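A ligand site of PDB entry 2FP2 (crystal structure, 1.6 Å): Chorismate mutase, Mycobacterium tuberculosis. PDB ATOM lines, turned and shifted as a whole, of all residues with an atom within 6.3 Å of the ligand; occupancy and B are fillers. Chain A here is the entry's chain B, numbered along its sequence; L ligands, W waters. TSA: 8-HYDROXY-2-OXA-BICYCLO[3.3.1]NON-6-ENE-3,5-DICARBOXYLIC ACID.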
ATOM      1  N   ARG A  16      -3.071   3.759  14.034  1.00  0.00           N
ATOM      2  CA  ARG A  16      -4.492   4.005  13.976  1.00  0.00           C
ATOM      3  C   ARG A  16      -4.728   5.529  14.009  1.00  0.00           C
ATOM      4  O   ARG A  16      -5.661   6.000  13.343  1.00  0.00           O
ATOM      5  CB  ARG A  16      -5.203   3.364  15.148  1.00  0.00           C
ATOM      6  CG  ARG A  16      -6.684   3.219  15.002  1.00  0.00           C
ATOM      7  CD  ARG A  16      -7.323   3.052  16.374  1.00  0.00           C
ATOM      8  NE  ARG A  16      -8.737   2.777  16.434  1.00  0.00           N
ATOM      9  CZ  ARG A  16      -9.707   3.687  16.437  1.00  0.00           C
ATOM     10  NH1 ARG A  16      -9.390   4.962  16.304  1.00  0.00           N
ATOM     11  NH2 ARG A  16     -10.965   3.317  16.577  1.00  0.00           N
ATOM     12  N   VAL A  23      -9.245   9.942   6.802  1.00  0.00           N
ATOM     13  CA  VAL A  23     -10.616  10.045   7.227  1.00  0.00           C
ATOM     14  C   VAL A  23     -11.034  11.532   7.129  1.00  0.00           C
ATOM     15  O   VAL A  23     -12.101  11.853   6.581  1.00  0.00           O
ATOM     16  CB  VAL A  23     -10.831   9.533   8.647  1.00  0.00           C
ATOM     17  CG1 VAL A  23     -12.190   9.971   9.220  1.00  0.00           C
ATOM     18  CG2 VAL A  23     -10.756   7.985   8.662  1.00  0.00           C
ATOM     19  N   LYS A  27     -13.919  13.341   4.753  1.00  0.00           N
ATOM     20  CA  LYS A  27     -15.016  14.094   5.319  1.00  0.00           C
ATOM     21  C   LYS A  27     -15.009  15.534   4.828  1.00  0.00           C
ATOM     22  O   LYS A  27     -16.078  16.156   4.690  1.00  0.00           O
ATOM     23  CB  LYS A  27     -14.965  14.058   6.846  1.00  0.00           C
ATOM     24  CG  LYS A  27     -15.219  12.691   7.369  1.00  0.00           C
ATOM     25  CD  LYS A  27     -15.062  12.661   8.870  1.00  0.00           C
ATOM     26  CE  LYS A  27     -15.477  11.322   9.417  1.00  0.00           C
ATOM     27  NZ  LYS A  27     -15.189  11.190  10.911  1.00  0.00           N
ATOM     28  N   PRO A  33     -19.673  15.717   9.027  1.00  0.00           N
ATOM     29  CA  PRO A  33     -19.128  16.008  10.355  1.00  0.00           C
ATOM     30  C   PRO A  33     -17.956  15.103  10.742  1.00  0.00           C
ATOM     31  O   PRO A  33     -17.836  13.974  10.255  1.00  0.00           O
ATOM     32  CB  PRO A  33     -20.307  15.728  11.302  1.00  0.00           C
ATOM     33  CG  PRO A  33     -21.532  15.793  10.456  1.00  0.00           C
ATOM     34  CD  PRO A  33     -21.111  15.414   9.068  1.00  0.00           C
ATOM     35  N   ILE A  34     -17.135  15.601  11.647  1.00  0.00           N
ATOM     36  CA  ILE A  34     -15.990  14.840  12.152  1.00  0.00           C
ATOM     37  C   ILE A  34     -16.446  13.786  13.122  1.00  0.00           C
ATOM     38  O   ILE A  34     -16.004  12.629  13.047  1.00  0.00           O
ATOM     39  CB  ILE A  34     -14.946  15.766  12.813  1.00  0.00           C
ATOM     40  CG1 ILE A  34     -14.116  16.427  11.703  1.00  0.00           C
ATOM     41  CG2 ILE A  34     -13.987  15.001  13.741  1.00  0.00           C
ATOM     42  CD1 ILE A  34     -13.428  17.642  12.111  1.00  0.00           C
ATOM     43  N   GLU A  35     -17.311  14.164  14.064  1.00  0.00           N
ATOM     44  CA  GLU A  35     -17.807  13.214  15.044  1.00  0.00           C
ATOM     45  C   GLU A  35     -18.967  12.389  14.478  1.00  0.00           C
ATOM     46  O   GLU A  35     -19.910  12.926  13.859  1.00  0.00           O
ATOM     47  CB  GLU A  35     -18.165  13.924  16.345  1.00  0.00           C
ATOM     48  CG  GLU A  35     -16.944  14.556  16.950  1.00  0.00           C
ATOM     49  CD  GLU A  35     -17.172  15.122  18.321  1.00  0.00           C
ATOM     50  OE1 GLU A  35     -16.684  16.237  18.580  1.00  0.00           O
ATOM     51  OE2 GLU A  35     -17.841  14.445  19.141  1.00  0.00           O
ATOM     52  N   ASP A  36     -18.860  11.077  14.636  1.00  0.00           N
ATOM     53  CA  ASP A  36     -19.882  10.131  14.187  1.00  0.00           C
ATOM     54  C   ASP A  36     -20.208   9.247  15.372  1.00  0.00           C
ATOM     55  O   ASP A  36     -19.579   8.203  15.598  1.00  0.00           O
ATOM     56  CB  ASP A  36     -19.377   9.301  13.016  1.00  0.00           C
ATOM     57  CG  ASP A  36     -20.468   8.434  12.385  1.00  0.00           C
ATOM     58  OD1 ASP A  36     -21.380   7.963  13.109  1.00  0.00           O
ATOM     59  OD2 ASP A  36     -20.413   8.233  11.152  1.00  0.00           O
ATOM     60  N   SER A  37     -21.186   9.692  16.155  1.00  0.00           N
ATOM     61  CA  SER A  37     -21.517   9.014  17.412  1.00  0.00           C
ATOM     62  C   SER A  37     -21.976   7.570  17.179  1.00  0.00           C
ATOM     63  O   SER A  37     -21.714   6.685  17.993  1.00  0.00           O
ATOM     64  CB  SER A  37     -22.573   9.797  18.206  1.00  0.00           C
ATOM     65  OG  SER A  37     -23.746   9.936  17.423  1.00  0.00           O
ATOM     66  N   ARG A  39     -20.880   5.452  14.820  1.00  0.00           N
ATOM     67  CA  ARG A  39     -19.675   4.656  14.595  1.00  0.00           C
ATOM     68  C   ARG A  39     -18.850   4.448  15.892  1.00  0.00           C
ATOM     69  O   ARG A  39     -18.309   3.369  16.147  1.00  0.00           O
ATOM     70  CB  ARG A  39     -18.836   5.315  13.496  1.00  0.00           C
ATOM     71  CG  ARG A  39     -17.454   4.768  13.341  1.00  0.00           C
ATOM     72  CD  ARG A  39     -17.411   3.264  12.949  1.00  0.00           C
ATOM     73  NE  ARG A  39     -16.028   2.863  12.751  1.00  0.00           N
ATOM     74  CZ  ARG A  39     -15.592   1.632  12.472  1.00  0.00           C
ATOM     75  NH1 ARG A  39     -16.457   0.631  12.362  1.00  0.00           N
ATOM     76  NH2 ARG A  39     -14.305   1.422  12.323  1.00  0.00           N
ATOM     77  N   VAL A  40     -18.762   5.480  16.729  1.00  0.00           N
ATOM     78  CA  VAL A  40     -18.111   5.336  18.037  1.00  0.00           C
ATOM     79  C   VAL A  40     -18.846   4.257  18.879  1.00  0.00           C
ATOM     80  O   VAL A  40     -18.226   3.355  19.467  1.00  0.00           O
ATOM     81  CB  VAL A  40     -18.078   6.688  18.778  1.00  0.00           C
ATOM     82  CG1 VAL A  40     -17.603   6.526  20.217  1.00  0.00           C
ATOM     83  CG2 VAL A  40     -17.182   7.680  18.022  1.00  0.00           C
ATOM     84  N   GLN A  43     -18.220   0.650  17.577  1.00  0.00           N
ATOM     85  CA  GLN A  43     -16.892   0.123  17.925  1.00  0.00           C
ATOM     86  C   GLN A  43     -16.810  -0.239  19.379  1.00  0.00           C
ATOM     87  O   GLN A  43     -16.271  -1.290  19.718  1.00  0.00           O
ATOM     88  CB  GLN A  43     -15.798   1.125  17.587  1.00  0.00           C
ATOM     89  CG  GLN A  43     -15.602   1.350  16.118  1.00  0.00           C
ATOM     90  CD  GLN A  43     -14.555   2.383  15.872  1.00  0.00           C
ATOM     91  OE1 GLN A  43     -13.396   2.036  15.615  1.00  0.00           O
ATOM     92  NE2 GLN A  43     -14.910   3.651  16.013  1.00  0.00           N
ATOM     93  N   PHE A  65     -10.198   2.840  24.499  1.00  0.00           N
ATOM     94  CA  PHE A  65     -10.664   3.145  23.143  1.00  0.00           C
ATOM     95  C   PHE A  65     -11.346   4.504  23.093  1.00  0.00           C
ATOM     96  O   PHE A  65     -11.234   5.228  22.102  1.00  0.00           O
ATOM     97  CB  PHE A  65     -11.479   2.022  22.544  1.00  0.00           C
ATOM     98  CG  PHE A  65     -10.647   0.944  21.996  1.00  0.00           C
ATOM     99  CD1 PHE A  65     -10.118   1.029  20.701  1.00  0.00           C
ATOM    100  CD2 PHE A  65     -10.301  -0.127  22.779  1.00  0.00           C
ATOM    101  CE1 PHE A  65      -9.284   0.026  20.200  1.00  0.00           C
ATOM    102  CE2 PHE A  65      -9.478  -1.166  22.275  1.00  0.00           C
ATOM    103  CZ  PHE A  65      -8.970  -1.074  20.970  1.00  0.00           C
ATOM    104  N   GLN A  68      -8.509   6.783  22.606  1.00  0.00           N
ATOM    105  CA  GLN A  68      -7.990   6.658  21.268  1.00  0.00           C
ATOM    106  C   GLN A  68      -8.869   7.430  20.298  1.00  0.00           C
ATOM    107  O   GLN A  68      -8.365   8.133  19.445  1.00  0.00           O
ATOM    108  CB  GLN A  68      -7.924   5.171  20.860  1.00  0.00           C
ATOM    109  CG  GLN A  68      -7.400   4.961  19.450  1.00  0.00           C
ATOM    110  CD  GLN A  68      -5.916   5.103  19.329  1.00  0.00           C
ATOM    111  OE1 GLN A  68      -5.174   4.777  20.263  1.00  0.00           O
ATOM    112  NE2 GLN A  68      -5.440   5.558  18.151  1.00  0.00           N
ATOM    113  N   ILE A  69     -10.178   7.261  20.464  1.00  0.00           N
ATOM    114  CA  ILE A  69     -11.192   7.871  19.576  1.00  0.00           C
ATOM    115  C   ILE A  69     -11.177   9.401  19.713  1.00  0.00           C
ATOM    116  O   ILE A  69     -11.131  10.124  18.701  1.00  0.00           O
ATOM    117  CB  ILE A  69     -12.572   7.251  19.835  1.00  0.00           C
ATOM    118  CG1 ILE A  69     -12.592   5.812  19.335  1.00  0.00           C
ATOM    119  CG2 ILE A  69     -13.714   8.056  19.172  1.00  0.00           C
ATOM    120  CD1 ILE A  69     -13.837   5.030  19.854  1.00  0.00           C
ATOM    121  N   ARG A  70     -11.132   9.884  20.935  1.00  0.00           N
ATOM    122  CA  ARG A  70     -11.050  11.329  21.167  1.00  0.00           C
ATOM    123  C   ARG A  70      -9.781  11.932  20.521  1.00  0.00           C
ATOM    124  O   ARG A  70      -9.783  12.983  19.860  1.00  0.00           O
ATOM    125  CB  ARG A  70     -11.103  11.581  22.678  1.00  0.00           C
ATOM    126  CG  ARG A  70     -11.286  12.989  23.053  1.00  0.00           C
ATOM    127  CD  ARG A  70     -11.835  13.118  24.485  1.00  0.00           C
ATOM    128  NE  ARG A  70     -11.189  12.174  25.387  1.00  0.00           N
ATOM    129  CZ  ARG A  70     -10.028  12.368  26.016  1.00  0.00           C
ATOM    130  NH1 ARG A  70      -9.334  13.504  25.918  1.00  0.00           N
ATOM    131  NH2 ARG A  70      -9.548  11.416  26.795  1.00  0.00           N
ATOM    132  N   THR A  72      -8.233  10.822  17.971  1.00  0.00           N
ATOM    133  CA  THR A  72      -8.420  10.711  16.527  1.00  0.00           C
ATOM    134  C   THR A  72      -9.245  11.906  16.059  1.00  0.00           C
ATOM    135  O   THR A  72      -8.881  12.572  15.096  1.00  0.00           O
ATOM    136  CB  THR A  72      -9.086   9.378  16.165  1.00  0.00           C
ATOM    137  OG1 THR A  72      -8.284   8.309  16.721  1.00  0.00           O
ATOM    138  CG2 THR A  72      -9.165   9.166  14.634  1.00  0.00           C
ATOM    139  N   GLU A  73     -10.328  12.150  16.757  1.00  0.00           N
ATOM    140  CA  GLU A  73     -11.180  13.327  16.468  1.00  0.00           C
ATOM    141  C   GLU A  73     -10.375  14.609  16.589  1.00  0.00           C
ATOM    142  O   GLU A  73     -10.508  15.515  15.750  1.00  0.00           O
ATOM    143  CB  GLU A  73     -12.409  13.341  17.357  1.00  0.00           C
ATOM    144  CG  GLU A  73     -13.337  12.211  17.092  1.00  0.00           C
ATOM    145  CD  GLU A  73     -14.366  11.910  18.154  1.00  0.00           C
ATOM    146  OE1 GLU A  73     -14.287  12.395  19.288  1.00  0.00           O
ATOM    147  OE2 GLU A  73     -15.256  11.108  17.820  1.00  0.00           O
ATOM    148  N   GLU A  76      -8.415  15.045  13.401  1.00  0.00           N
ATOM    149  CA  GLU A  76      -9.348  15.429  12.303  1.00  0.00           C
ATOM    150  C   GLU A  76      -9.696  16.928  12.402  1.00  0.00           C
ATOM    151  O   GLU A  76      -9.580  17.646  11.399  1.00  0.00           O
ATOM    152  CB  GLU A  76     -10.583  14.589  12.306  1.00  0.00           C
ATOM    153  CG  GLU A  76     -10.302  13.125  12.039  1.00  0.00           C
ATOM    154  CD  GLU A  76     -11.527  12.256  12.050  1.00  0.00           C
ATOM    155  OE1 GLU A  76     -12.546  12.621  11.423  1.00  0.00           O
ATOM    156  OE2 GLU A  76     -11.475  11.167  12.688  1.00  0.00           O
ATOM    157  N   LEU A  97     -14.129   6.310   3.118  1.00  0.00           N
ATOM    158  CA  LEU A  97     -14.317   6.181   4.562  1.00  0.00           C
ATOM    159  C   LEU A  97     -14.484   4.695   4.949  1.00  0.00           C
ATOM    160  O   LEU A  97     -13.923   4.229   5.957  1.00  0.00           O
ATOM    161  CB  LEU A  97     -15.538   6.993   4.986  1.00  0.00           C
ATOM    162  CG  LEU A  97     -15.834   7.140   6.476  1.00  0.00           C
ATOM    163  CD1 LEU A  97     -14.598   7.620   7.263  1.00  0.00           C
ATOM    164  CD2 LEU A  97     -17.012   8.066   6.689  1.00  0.00           C
ATOM    165  N   ARG A 101     -12.298   2.789   7.649  1.00  0.00           N
ATOM    166  CA  ARG A 101     -12.964   2.106   8.758  1.00  0.00           C
ATOM    167  C   ARG A 101     -12.568   0.628   8.828  1.00  0.00           C
ATOM    168  O   ARG A 101     -12.350   0.119   9.923  1.00  0.00           O
ATOM    169  CB  ARG A 101     -14.469   2.313   8.716  1.00  0.00           C
ATOM    170  CG  ARG A 101     -14.816   3.731   9.074  1.00  0.00           C
ATOM    171  CD  ARG A 101     -16.259   3.963   9.235  1.00  0.00           C
ATOM    172  NE  ARG A 101     -16.512   5.301   9.791  1.00  0.00           N
ATOM    173  CZ  ARG A 101     -17.708   5.864   9.861  1.00  0.00           C
ATOM    174  NH1 ARG A 101     -18.770   5.211   9.383  1.00  0.00           N
ATOM    175  NH2 ARG A 101     -17.839   7.075  10.379  1.00  0.00           N
ATOM    176  N   ILE A 104      -9.177   0.601  10.371  1.00  0.00           N
ATOM    177  CA  ILE A 104      -9.384   0.860  11.829  1.00  0.00           C
ATOM    178  C   ILE A 104      -9.891  -0.379  12.568  1.00  0.00           C
ATOM    179  O   ILE A 104      -9.436  -0.682  13.675  1.00  0.00           O
ATOM    180  CB  ILE A 104     -10.307   2.096  12.093  1.00  0.00           C
ATOM    181  CG1 ILE A 104      -9.511   3.346  11.793  1.00  0.00           C
ATOM    182  CG2 ILE A 104     -10.862   2.059  13.544  1.00  0.00           C
ATOM    183  CD1 ILE A 104     -10.391   4.627  11.683  1.00  0.00           C
ATOM    184  N   ASN A 108      -8.083  -1.944  15.717  1.00  0.00           N
ATOM    185  CA  ASN A 108      -8.840  -2.194  16.951  1.00  0.00           C
ATOM    186  C   ASN A 108      -8.512  -3.597  17.477  1.00  0.00           C
ATOM    187  O   ASN A 108      -8.149  -3.795  18.643  1.00  0.00           O
ATOM    188  CB  ASN A 108     -10.357  -2.080  16.761  1.00  0.00           C
ATOM    189  CG  ASN A 108     -10.828  -0.648  16.549  1.00  0.00           C
ATOM    190  OD1 ASN A 108     -10.059   0.327  16.746  1.00  0.00           O
ATOM    191  ND2 ASN A 108     -12.123  -0.495  16.176  1.00  0.00           N
HETATM  192  C1  TSA L   1     -13.291   7.556  14.710  1.00  0.00           C
HETATM  193  C2  TSA L   1     -14.763   7.147  14.724  1.00  0.00           C
HETATM  194  C3  TSA L   1     -15.767   8.026  14.609  1.00  0.00           C
HETATM  195  C4  TSA L   1     -15.547   9.523  14.413  1.00  0.00           C
HETATM  196  O5  TSA L   1     -16.169  10.240  15.461  1.00  0.00           O
HETATM  197  C5  TSA L   1     -14.063   9.877  14.306  1.00  0.00           C
HETATM  198  C6  TSA L   1     -13.175   9.014  15.191  1.00  0.00           C
HETATM  199  O7  TSA L   1     -13.641   9.724  12.933  1.00  0.00           O
HETATM  200  C8  TSA L   1     -13.371   8.441  12.324  1.00  0.00           C
HETATM  201  C9  TSA L   1     -12.706   7.474  13.316  1.00  0.00           C
HETATM  202  C10 TSA L   1     -12.426   6.602  15.500  1.00  0.00           C
HETATM  203  O1  TSA L   1     -11.427   7.054  16.118  1.00  0.00           O
HETATM  204  O2  TSA L   1     -12.724   5.372  15.463  1.00  0.00           O
HETATM  205  C11 TSA L   1     -14.582   7.821  11.667  1.00  0.00           C
HETATM  206  O3  TSA L   1     -14.567   6.552  11.490  1.00  0.00           O
HETATM  207  O4  TSA L   1     -15.566   8.542  11.340  1.00  0.00           O
HETATM  208  O   HOH W   1     -13.653   4.391  12.949  1.00  0.00           O
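Water W1 lies within hydrogen-bond range of O3 of the ligand, NE of Arg 39 and NE2 of Gln 43.
The guanidinium group of Arg 16 lies within hydrogen-bond range of the side-chain amide oxygen of Asn 108, 2.8 Å away. OE1 of Gln 43 lies within hydrogen-bond range of ND2 of Asn 108 (2.9 Å). O of Arg 39 sits close to NE2 of Gln 43, at 3.4 Å. NZ of Lys 27 sits at hydrogen-bond distance from O of Ile 34, 2.7 Å away. The side-chain amino group of Lys 27 is in salt-bridge range of the side-chain carboxylate of Glu 76. The side-chain carboxylate (OD1) of Asp 36 lies within hydrogen-bond range of the backbone NH (N) of Arg 39, 3.1 Å away. The side-chain hydroxyl of Thr 72 is in hydrogen-bond range of the backbone carbonyl oxygen of Gln 68 (2.7 Å). OE1 of Gln 43 is in hydrogen-bond range of NH2 of Arg 16 (2.9 Å).
Val 23 touches the ligand. Glu 35 touches the ligand. Arg 39 touches the ligand (CG to C2, 3.8 Å). Val 40 touches the ligand (CG2 to C3, 3.7 Å). CA of Ile 69 touches O1 of the ligand (3.6 Å). Hydrophobic or aromatic side chains that line the ligand: Val 23, Val 40 and Ile 69. The nearest printed residue that does not touch the ligand is Ile 104 (4.02 Å).
NH1 of Arg 16 is in salt-bridge range of O1 of the ligand. OE2 of Glu 73 sits at hydrogen-bond distance from O5 of the ligand. The side-chain amide nitrogen (NE2) of Gln 43 lies within hydrogen-bond range of an oxygen (O2) of the ligand, at 2.8 Å. The side-chain amino group of Lys 27 is in salt-bridge range of an oxygen (O4) of the ligand, at 2.7 Å. The backbone carbonyl oxygen of Ile 34 sits at hydrogen-bond distance from an oxygen (O5) of the ligand, at 3.4 Å. The guanidinium group of Arg 101 lies within salt-bridge range of an oxygen (O3) of the ligand (2.9 Å). The side-chain carboxylate (OE2) of Glu 76 lies close to an oxygen (O7) of the ligand, 2.6 Å away. OG1 of Thr 72 lies close to O1 of the ligand (3.4 Å). The backbone NH (N) of Asp 36 is in hydrogen-bond range of an oxygen (O5) of the ligand (2.9 Å).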
